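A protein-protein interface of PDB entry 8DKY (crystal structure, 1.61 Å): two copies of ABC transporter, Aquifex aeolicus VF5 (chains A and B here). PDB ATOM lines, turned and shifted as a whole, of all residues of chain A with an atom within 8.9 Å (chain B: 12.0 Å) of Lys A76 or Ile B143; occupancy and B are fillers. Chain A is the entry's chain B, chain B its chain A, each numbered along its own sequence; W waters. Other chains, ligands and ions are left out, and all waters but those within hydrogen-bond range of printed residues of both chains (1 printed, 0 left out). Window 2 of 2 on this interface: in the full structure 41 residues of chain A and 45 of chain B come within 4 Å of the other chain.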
ATOM      1  N   VAL A   7      31.731 -11.724  21.389  1.00  0.00           N
ATOM      2  CA  VAL A   7      32.812 -12.701  21.338  1.00  0.00           C
ATOM      3  C   VAL A   7      32.234 -14.077  21.045  1.00  0.00           C
ATOM      4  O   VAL A   7      31.186 -14.451  21.584  1.00  0.00           O
ATOM      5  CB  VAL A   7      33.624 -12.728  22.653  1.00  0.00           C
ATOM      6  CG1 VAL A   7      34.916 -13.514  22.468  1.00  0.00           C
ATOM      7  CG2 VAL A   7      33.931 -11.315  23.131  1.00  0.00           C
ATOM      8  N   LYS A   9      32.762 -17.572  22.023  1.00  0.00           N
ATOM      9  CA  LYS A   9      33.454 -18.205  23.139  1.00  0.00           C
ATOM     10  C   LYS A   9      33.883 -19.629  22.819  1.00  0.00           C
ATOM     11  O   LYS A   9      34.880 -20.107  23.371  1.00  0.00           O
ATOM     12  CB  LYS A   9      32.566 -18.191  24.383  1.00  0.00           C
ATOM     13  CG  LYS A   9      32.402 -16.813  24.999  1.00  0.00           C
ATOM     14  CD  LYS A   9      33.361 -16.602  26.156  1.00  0.00           C
ATOM     15  CE  LYS A   9      33.170 -15.229  26.776  1.00  0.00           C
ATOM     16  NZ  LYS A   9      34.386 -14.771  27.501  1.00  0.00           N
ATOM     17  N   ARG A  12      31.657 -25.633  18.198  1.00  0.00           N
ATOM     18  CA  ARG A  12      31.548 -27.084  18.221  1.00  0.00           C
ATOM     19  C   ARG A  12      30.958 -27.577  16.910  1.00  0.00           C
ATOM     20  O   ARG A  12      29.986 -27.010  16.400  1.00  0.00           O
ATOM     21  CB  ARG A  12      30.687 -27.572  19.396  1.00  0.00           C
ATOM     22  CG  ARG A  12      31.271 -27.267  20.767  1.00  0.00           C
ATOM     23  CD  ARG A  12      30.324 -27.689  21.881  1.00  0.00           C
ATOM     24  NE  ARG A  12      29.042 -26.990  21.824  1.00  0.00           N
ATOM     25  CZ  ARG A  12      28.802 -25.818  22.406  1.00  0.00           C
ATOM     26  NH1 ARG A  12      29.757 -25.209  23.095  1.00  0.00           N
ATOM     27  NH2 ARG A  12      27.606 -25.256  22.303  1.00  0.00           N
ATOM     28  N   GLU A  32      27.803 -25.126  16.005  1.00  0.00           N
ATOM     29  CA  GLU A  32      27.338 -24.426  17.192  1.00  0.00           C
ATOM     30  C   GLU A  32      28.386 -23.401  17.603  1.00  0.00           C
ATOM     31  O   GLU A  32      29.580 -23.712  17.642  1.00  0.00           O
ATOM     32  CB  GLU A  32      27.076 -25.417  18.330  1.00  0.00           C
ATOM     33  CG  GLU A  32      25.842 -26.283  18.116  1.00  0.00           C
ATOM     34  CD  GLU A  32      25.543 -27.205  19.283  1.00  0.00           C
ATOM     35  OE1 GLU A  32      26.450 -27.441  20.111  1.00  0.00           O
ATOM     36  OE2 GLU A  32      24.400 -27.700  19.367  1.00  0.00           O
ATOM     37  N   LEU A  33      27.941 -22.178  17.890  1.00  0.00           N
ATOM     38  CA  LEU A  33      28.820 -21.104  18.338  1.00  0.00           C
ATOM     39  C   LEU A  33      28.242 -20.508  19.612  1.00  0.00           C
ATOM     40  O   LEU A  33      27.117 -19.999  19.606  1.00  0.00           O
ATOM     41  CB  LEU A  33      28.982 -20.017  17.265  1.00  0.00           C
ATOM     42  CG  LEU A  33      29.452 -20.425  15.864  1.00  0.00           C
ATOM     43  CD1 LEU A  33      28.282 -20.757  14.948  1.00  0.00           C
ATOM     44  CD2 LEU A  33      30.320 -19.336  15.250  1.00  0.00           C
ATOM     45  N   ASP A  34      29.003 -20.594  20.702  1.00  0.00           N
ATOM     46  CA  ASP A  34      28.642 -19.946  21.956  1.00  0.00           C
ATOM     47  C   ASP A  34      29.072 -18.486  21.892  1.00  0.00           C
ATOM     48  O   ASP A  34      30.268 -18.193  21.794  1.00  0.00           O
ATOM     49  CB  ASP A  34      29.316 -20.656  23.128  1.00  0.00           C
ATOM     50  CG  ASP A  34      28.701 -22.011  23.427  1.00  0.00           C
ATOM     51  OD1 ASP A  34      27.790 -22.436  22.688  1.00  0.00           O
ATOM     52  OD2 ASP A  34      29.135 -22.657  24.405  1.00  0.00           O
ATOM     53  N   VAL A  35      28.105 -17.571  21.941  1.00  0.00           N
ATOM     54  CA  VAL A  35      28.347 -16.151  21.717  1.00  0.00           C
ATOM     55  C   VAL A  35      27.967 -15.389  22.979  1.00  0.00           C
ATOM     56  O   VAL A  35      26.978 -15.720  23.637  1.00  0.00           O
ATOM     57  CB  VAL A  35      27.547 -15.641  20.499  1.00  0.00           C
ATOM     58  CG1 VAL A  35      27.517 -14.121  20.457  1.00  0.00           C
ATOM     59  CG2 VAL A  35      28.116 -16.213  19.201  1.00  0.00           C
ATOM     60  N   GLU A  36      28.764 -14.387  23.337  1.00  0.00           N
ATOM     61  CA  GLU A  36      28.421 -13.507  24.447  1.00  0.00           C
ATOM     62  C   GLU A  36      28.547 -12.065  23.984  1.00  0.00           C
ATOM     63  O   GLU A  36      29.603 -11.655  23.492  1.00  0.00           O
ATOM     64  CB  GLU A  36      29.298 -13.781  25.673  1.00  0.00           C
ATOM     65  CG  GLU A  36      29.094 -15.186  26.238  1.00  0.00           C
ATOM     66  CD  GLU A  36      29.752 -15.401  27.588  1.00  0.00           C
ATOM     67  OE1 GLU A  36      30.154 -14.406  28.228  1.00  0.00           O
ATOM     68  OE2 GLU A  36      29.871 -16.573  28.004  1.00  0.00           O
ATOM     69  N   ALA A  37      27.460 -11.313  24.118  1.00  0.00           N
ATOM     70  CA  ALA A  37      27.426  -9.897  23.785  1.00  0.00           C
ATOM     71  C   ALA A  37      27.690  -9.092  25.051  1.00  0.00           C
ATOM     72  O   ALA A  37      26.928  -9.186  26.023  1.00  0.00           O
ATOM     73  CB  ALA A  37      26.080  -9.513  23.173  1.00  0.00           C
ATOM     74  N   LYS A  38      28.777  -8.311  25.030  1.00  0.00           N
ATOM     75  CA  LYS A  38      29.160  -7.457  26.148  1.00  0.00           C
ATOM     76  C   LYS A  38      28.305  -6.203  26.239  1.00  0.00           C
ATOM     77  O   LYS A  38      28.297  -5.546  27.287  1.00  0.00           O
ATOM     78  CB  LYS A  38      30.629  -7.052  26.014  1.00  0.00           C
ATOM     79  CG  LYS A  38      31.610  -8.209  26.048  1.00  0.00           C
ATOM     80  CD  LYS A  38      33.040  -7.699  26.016  1.00  0.00           C
ATOM     81  CE  LYS A  38      34.039  -8.844  25.986  1.00  0.00           C
ATOM     82  NZ  LYS A  38      35.440  -8.352  25.889  1.00  0.00           N
ATOM     83  N   GLU A  39      27.613  -5.847  25.159  1.00  0.00           N
ATOM     84  CA  GLU A  39      26.716  -4.703  25.132  1.00  0.00           C
ATOM     85  C   GLU A  39      25.609  -5.012  24.136  1.00  0.00           C
ATOM     86  O   GLU A  39      25.689  -5.979  23.372  1.00  0.00           O
ATOM     87  CB  GLU A  39      27.452  -3.417  24.740  1.00  0.00           C
ATOM     88  CG  GLU A  39      28.327  -3.569  23.504  1.00  0.00           C
ATOM     89  CD  GLU A  39      28.993  -2.271  23.088  1.00  0.00           C
ATOM     90  OE1 GLU A  39      28.317  -1.421  22.470  1.00  0.00           O
ATOM     91  OE2 GLU A  39      30.201  -2.108  23.362  1.00  0.00           O
ATOM     92  N   LEU A  72      21.386  -8.485  19.239  1.00  0.00           N
ATOM     93  CA  LEU A  72      21.901  -9.048  20.479  1.00  0.00           C
ATOM     94  C   LEU A  72      21.707  -8.063  21.621  1.00  0.00           C
ATOM     95  O   LEU A  72      22.181  -6.924  21.555  1.00  0.00           O
ATOM     96  CB  LEU A  72      23.374  -9.427  20.340  1.00  0.00           C
ATOM     97  CG  LEU A  72      23.680 -10.386  19.190  1.00  0.00           C
ATOM     98  CD1 LEU A  72      25.127 -10.841  19.237  1.00  0.00           C
ATOM     99  CD2 LEU A  72      22.739 -11.580  19.239  1.00  0.00           C
ATOM    100  N   LYS A  73      20.997  -8.501  22.652  1.00  0.00           N
ATOM    101  CA  LYS A  73      21.034  -7.843  23.945  1.00  0.00           C
ATOM    102  C   LYS A  73      22.193  -8.428  24.739  1.00  0.00           C
ATOM    103  O   LYS A  73      22.549  -9.597  24.571  1.00  0.00           O
ATOM    104  CB  LYS A  73      19.721  -8.041  24.702  1.00  0.00           C
ATOM    105  CG  LYS A  73      18.474  -7.756  23.878  1.00  0.00           C
ATOM    106  CD  LYS A  73      18.386  -6.295  23.471  1.00  0.00           C
ATOM    107  CE  LYS A  73      17.272  -6.078  22.458  1.00  0.00           C
ATOM    108  NZ  LYS A  73      17.221  -4.668  21.985  1.00  0.00           N
ATOM    109  N   LYS A  74      22.801  -7.595  25.582  1.00  0.00           N
ATOM    110  CA  LYS A  74      23.880  -8.040  26.457  1.00  0.00           C
ATOM    111  C   LYS A  74      23.518  -9.352  27.141  1.00  0.00           C
ATOM    112  O   LYS A  74      22.489  -9.449  27.816  1.00  0.00           O
ATOM    113  CB  LYS A  74      24.169  -6.966  27.507  1.00  0.00           C
ATOM    114  CG  LYS A  74      25.469  -7.165  28.261  1.00  0.00           C
ATOM    115  CD  LYS A  74      25.565  -6.205  29.438  1.00  0.00           C
ATOM    116  CE  LYS A  74      26.949  -6.224  30.060  1.00  0.00           C
ATOM    117  NZ  LYS A  74      27.085  -7.355  31.017  1.00  0.00           N
ATOM    118  N   GLY A  75      24.354 -10.366  26.947  1.00  0.00           N
ATOM    119  CA  GLY A  75      24.074 -11.677  27.507  1.00  0.00           C
ATOM    120  C   GLY A  75      24.635 -12.780  26.628  1.00  0.00           C
ATOM    121  O   GLY A  75      25.490 -12.543  25.785  1.00  0.00           O
ATOM    122  N   LYS A  76      24.127 -13.993  26.839  1.00  0.00           N
ATOM    123  CA  LYS A  76      24.663 -15.192  26.206  1.00  0.00           C
ATOM    124  C   LYS A  76      23.693 -15.760  25.176  1.00  0.00           C
ATOM    125  O   LYS A  76      22.471 -15.677  25.331  1.00  0.00           O
ATOM    126  CB  LYS A  76      24.983 -16.263  27.252  1.00  0.00           C
ATOM    127  CG  LYS A  76      25.980 -15.825  28.312  1.00  0.00           C
ATOM    128  CD  LYS A  76      26.284 -16.972  29.262  1.00  0.00           C
ATOM    129  CE  LYS A  76      27.518 -16.698  30.103  1.00  0.00           C
ATOM    130  NZ  LYS A  76      27.807 -17.825  31.033  1.00  0.00           N
ATOM    131  N   TYR A  77      24.258 -16.350  24.120  1.00  0.00           N
ATOM    132  CA  TYR A  77      23.508 -16.866  22.985  1.00  0.00           C
ATOM    133  C   TYR A  77      24.159 -18.132  22.448  1.00  0.00           C
ATOM    134  O   TYR A  77      25.367 -18.343  22.591  1.00  0.00           O
ATOM    135  CB  TYR A  77      23.427 -15.858  21.828  1.00  0.00           C
ATOM    136  CG  TYR A  77      22.664 -14.591  22.118  1.00  0.00           C
ATOM    137  CD1 TYR A  77      23.207 -13.593  22.916  1.00  0.00           C
ATOM    138  CD2 TYR A  77      21.405 -14.384  21.576  1.00  0.00           C
ATOM    139  CE1 TYR A  77      22.512 -12.436  23.178  1.00  0.00           C
ATOM    140  CE2 TYR A  77      20.705 -13.227  21.826  1.00  0.00           C
ATOM    141  CZ  TYR A  77      21.260 -12.257  22.633  1.00  0.00           C
ATOM    142  OH  TYR A  77      20.564 -11.098  22.894  1.00  0.00           O
ATOM    143  N   LEU A  78      23.342 -18.956  21.796  1.00  0.00           N
ATOM    144  CA  LEU A  78      23.804 -20.067  20.972  1.00  0.00           C
ATOM    145  C   LEU A  78      23.413 -19.778  19.529  1.00  0.00           C
ATOM    146  O   LEU A  78      22.222 -19.654  19.221  1.00  0.00           O
ATOM    147  CB  LEU A  78      23.196 -21.391  21.434  1.00  0.00           C
ATOM    148  CG  LEU A  78      23.455 -22.652  20.602  1.00  0.00           C
ATOM    149  CD1 LEU A  78      24.942 -22.978  20.532  1.00  0.00           C
ATOM    150  CD2 LEU A  78      22.659 -23.836  21.141  1.00  0.00           C
ATOM    151  N   PHE A  79      24.409 -19.646  18.656  1.00  0.00           N
ATOM    152  CA  PHE A  79      24.187 -19.547  17.220  1.00  0.00           C
ATOM    153  C   PHE A  79      24.359 -20.929  16.607  1.00  0.00           C
ATOM    154  O   PHE A  79      25.257 -21.678  16.999  1.00  0.00           O
ATOM    155  CB  PHE A  79      25.170 -18.574  16.554  1.00  0.00           C
ATOM    156  CG  PHE A  79      24.939 -17.114  16.878  1.00  0.00           C
ATOM    157  CD1 PHE A  79      24.223 -16.716  17.996  1.00  0.00           C
ATOM    158  CD2 PHE A  79      25.453 -16.135  16.040  1.00  0.00           C
ATOM    159  CE1 PHE A  79      24.030 -15.370  18.270  1.00  0.00           C
ATOM    160  CE2 PHE A  79      25.260 -14.793  16.305  1.00  0.00           C
ATOM    161  CZ  PHE A  79      24.549 -14.409  17.423  1.00  0.00           C
ATOM    162  N   THR A  80      23.508 -21.268  15.640  1.00  0.00           N
ATOM    163  CA  THR A  80      23.598 -22.576  15.001  1.00  0.00           C
ATOM    164  C   THR A  80      23.452 -22.443  13.493  1.00  0.00           C
ATOM    165  O   THR A  80      22.533 -21.775  13.008  1.00  0.00           O
ATOM    166  CB  THR A  80      22.535 -23.540  15.545  1.00  0.00           C
ATOM    167  OG1 THR A  80      22.654 -23.634  16.970  1.00  0.00           O
ATOM    168  CG2 THR A  80      22.716 -24.926  14.941  1.00  0.00           C
ATOM    169  N   PHE B 138      19.916 -21.156   9.533  1.00  0.00           N
ATOM    170  CA  PHE B 138      20.479 -20.412  10.653  1.00  0.00           C
ATOM    171  C   PHE B 138      19.401 -20.137  11.693  1.00  0.00           C
ATOM    172  O   PHE B 138      18.219 -20.001  11.366  1.00  0.00           O
ATOM    173  CB  PHE B 138      21.115 -19.080  10.200  1.00  0.00           C
ATOM    174  CG  PHE B 138      21.544 -18.192  11.338  1.00  0.00           C
ATOM    175  CD1 PHE B 138      22.739 -18.423  12.004  1.00  0.00           C
ATOM    176  CD2 PHE B 138      20.750 -17.133  11.747  1.00  0.00           C
ATOM    177  CE1 PHE B 138      23.135 -17.613  13.054  1.00  0.00           C
ATOM    178  CE2 PHE B 138      21.141 -16.319  12.797  1.00  0.00           C
ATOM    179  CZ  PHE B 138      22.336 -16.561  13.450  1.00  0.00           C
ATOM    180  N   ASN B 139      19.823 -20.069  12.956  1.00  0.00           N
ATOM    181  CA  ASN B 139      18.957 -19.642  14.047  1.00  0.00           C
ATOM    182  C   ASN B 139      19.832 -19.231  15.223  1.00  0.00           C
ATOM    183  O   ASN B 139      20.963 -19.704  15.372  1.00  0.00           O
ATOM    184  CB  ASN B 139      17.963 -20.745  14.451  1.00  0.00           C
ATOM    185  CG  ASN B 139      18.582 -21.807  15.352  1.00  0.00           C
ATOM    186  OD1 ASN B 139      18.851 -21.568  16.530  1.00  0.00           O
ATOM    187  ND2 ASN B 139      18.808 -22.991  14.796  1.00  0.00           N
ATOM    188  N   TYR B 140      19.300 -18.338  16.058  1.00  0.00           N
ATOM    189  CA  TYR B 140      19.977 -17.974  17.293  1.00  0.00           C
ATOM    190  C   TYR B 140      18.946 -17.832  18.404  1.00  0.00           C
ATOM    191  O   TYR B 140      17.756 -17.620  18.155  1.00  0.00           O
ATOM    192  CB  TYR B 140      20.802 -16.679  17.167  1.00  0.00           C
ATOM    193  CG  TYR B 140      20.017 -15.385  17.060  1.00  0.00           C
ATOM    194  CD1 TYR B 140      19.333 -15.043  15.900  1.00  0.00           C
ATOM    195  CD2 TYR B 140      19.993 -14.484  18.121  1.00  0.00           C
ATOM    196  CE1 TYR B 140      18.632 -13.847  15.809  1.00  0.00           C
ATOM    197  CE2 TYR B 140      19.298 -13.290  18.038  1.00  0.00           C
ATOM    198  CZ  TYR B 140      18.619 -12.976  16.882  1.00  0.00           C
ATOM    199  OH  TYR B 140      17.925 -11.788  16.797  1.00  0.00           O
ATOM    200  N   ARG B 141      19.435 -17.948  19.639  1.00  0.00           N
ATOM    201  CA  ARG B 141      18.633 -17.987  20.857  1.00  0.00           C
ATOM    202  C   ARG B 141      19.467 -17.583  22.059  1.00  0.00           C
ATOM    203  O   ARG B 141      20.626 -17.981  22.191  1.00  0.00           O
ATOM    204  CB  ARG B 141      18.034 -19.376  21.089  1.00  0.00           C
ATOM    205  CG  ARG B 141      16.941 -19.762  20.127  1.00  0.00           C
ATOM    206  CD  ARG B 141      16.650 -21.214  20.246  1.00  0.00           C
ATOM    207  NE  ARG B 141      17.898 -21.864  19.871  1.00  0.00           N
ATOM    208  CZ  ARG B 141      18.105 -23.171  19.813  1.00  0.00           C
ATOM    209  NH1 ARG B 141      19.293 -23.623  19.440  1.00  0.00           N
ATOM    210  NH2 ARG B 141      17.129 -24.023  20.090  1.00  0.00           N
ATOM    211  N   LYS B 142      18.850 -16.783  22.922  1.00  0.00           N
ATOM    212  CA  LYS B 142      19.429 -16.446  24.211  1.00  0.00           C
ATOM    213  C   LYS B 142      19.541 -17.695  25.076  1.00  0.00           C
ATOM    214  O   LYS B 142      18.695 -18.591  25.013  1.00  0.00           O
ATOM    215  CB  LYS B 142      18.547 -15.406  24.906  1.00  0.00           C
ATOM    216  CG  LYS B 142      18.581 -14.023  24.276  1.00  0.00           C
ATOM    217  CD  LYS B 142      17.684 -13.037  25.016  1.00  0.00           C
ATOM    218  CE  LYS B 142      17.138 -11.978  24.057  1.00  0.00           C
ATOM    219  NZ  LYS B 142      16.073 -11.120  24.658  1.00  0.00           N
ATOM    220  N   ILE B 143      20.595 -17.758  25.883  1.00  0.00           N
ATOM    221  CA  ILE B 143      20.757 -18.826  26.871  1.00  0.00           C
ATOM    222  C   ILE B 143      21.143 -18.209  28.211  1.00  0.00           C
ATOM    223  O   ILE B 143      21.965 -17.281  28.248  1.00  0.00           O
ATOM    224  CB  ILE B 143      21.783 -19.880  26.410  1.00  0.00           C
ATOM    225  CG1 ILE B 143      21.422 -20.440  25.031  1.00  0.00           C
ATOM    226  CG2 ILE B 143      21.935 -21.003  27.421  1.00  0.00           C
ATOM    227  CD1 ILE B 143      22.140 -21.734  24.706  1.00  0.00           C
ATOM    228  N   PRO B 144      20.562 -18.666  29.335  1.00  0.00           N
ATOM    229  CA  PRO B 144      20.972 -18.170  30.654  1.00  0.00           C
ATOM    230  C   PRO B 144      22.422 -18.502  30.990  1.00  0.00           C
ATOM    231  O   PRO B 144      22.891 -19.579  30.622  1.00  0.00           O
ATOM    232  CB  PRO B 144      20.013 -18.883  31.612  1.00  0.00           C
ATOM    233  CG  PRO B 144      19.566 -20.100  30.887  1.00  0.00           C
ATOM    234  CD  PRO B 144      19.554 -19.740  29.431  1.00  0.00           C
HETATM  235  O   HOH W   1      21.012 -21.771  18.285  1.00  0.00           O
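Among the printed residues, pairs that only touch across the chains: Lys A76 with Lys B142, Tyr A77 with Tyr B140, Tyr A77 with Arg B141, Tyr A77 with Lys B142, Leu A78 with Tyr B140, Leu A78 with Ile B143, Phe A79 with Asn B139, Phe A79 with Tyr B140 and Thr A80 with Phe B138.
The backbone carbonyl oxygen (O) of Asn B139 is in hydrogen-bond range of the backbone NH (N) of Thr A80 (3.0 Å). The backbone carbonyl oxygen (O) of Arg B141 sits at hydrogen-bond distance from the backbone NH (N) of Leu A78 (2.9 Å). The backbone NH of Ile B143 sits at hydrogen-bond distance from the backbone carbonyl oxygen of Lys A76, 2.9 Å away.
Water W1 lies within hydrogen-bond range of the backbone carbonyl oxygen of Leu A78 (2.6 Å), the guanidinium group of Arg B141 (2.8 Å), the side-chain amide oxygen of Asn B139 (2.8 Å) and the side-chain hydroxyl of Thr A80 (2.8 Å).
The side-chain amide oxygen (OD1) of Asn B139 lies within hydrogen-bond range of the guanidinium group (NE) of Arg B141 (3.5 Å). The backbone carbonyl oxygen (O) of Phe A79 lies within hydrogen-bond range of the backbone NH (N) of Leu A33. O of Val A35 lies within hydrogen-bond range of N of Tyr A77, at 2.8 Å. The side-chain carboxylate (OE2) of Glu A36 is in salt-bridge range of the side-chain amino group (NZ) of Lys A76 (3.9 Å). N of Lys A73 sits at hydrogen-bond distance from OH of Tyr A77.
Printed residues of chain A that touch a printed residue of chain B: Lys A76, Tyr A77, Leu A78, Phe A79 and Thr A80. Hydrophobic or aromatic side chains of chain A that line the printed part of chain B: Tyr A77, Leu A78 and Phe A79. Among the printed residues, no Asp or Glu carboxylate lies within 4 Å of a Lys or Arg side-chain nitrogen of the other chain.
Of chain B, only Lys B142 (3.3 Å) and Ile B143 (2.9 Å) come within 4 Å of Lys A76. Ile B143 touches just these residues of chain A: Lys A76 and Leu A78. No residue of chain B comes within 4 Å of Val A35. Glu A36 touches none of the printed residues of chain B. No residue of chain B comes within 4 Å of Ala A37. No residue of chain B comes within 4 Å of Gly A75. Of chain B, only Tyr B140 (3.7 Å), Arg B141 (3.2 Å) and Lys B142 (3.3 Å) come within 4 Å of Tyr A77. No residue of chain A comes within 4 Å of Pro B144. Of the printed residues of chain A, Arg B141 touches Tyr A77 (3.2 Å) and Leu A78 (2.9 Å). Printed residues of chain A within 4 Å of Lys B142: Lys A76 and Tyr A77. Printed residues of chain A within 4 Å of Asn B139: Phe A79 (3.7 Å) and Thr A80 (3.0 Å). Of the printed residues of chain A, Phe B138 touches Thr A80 (3.4 Å). Glu A39 touches none of the printed residues of chain B. Arg A12 touches none of the printed residues of chain B. The nearest residue of chain A that does not touch Ile B143 is Tyr A77 (4.2 Å).
No position is printed for both chains. Of the 12 pairs that touch across the chains among the printed residues, none has its exchanged pair printed and touching as well.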
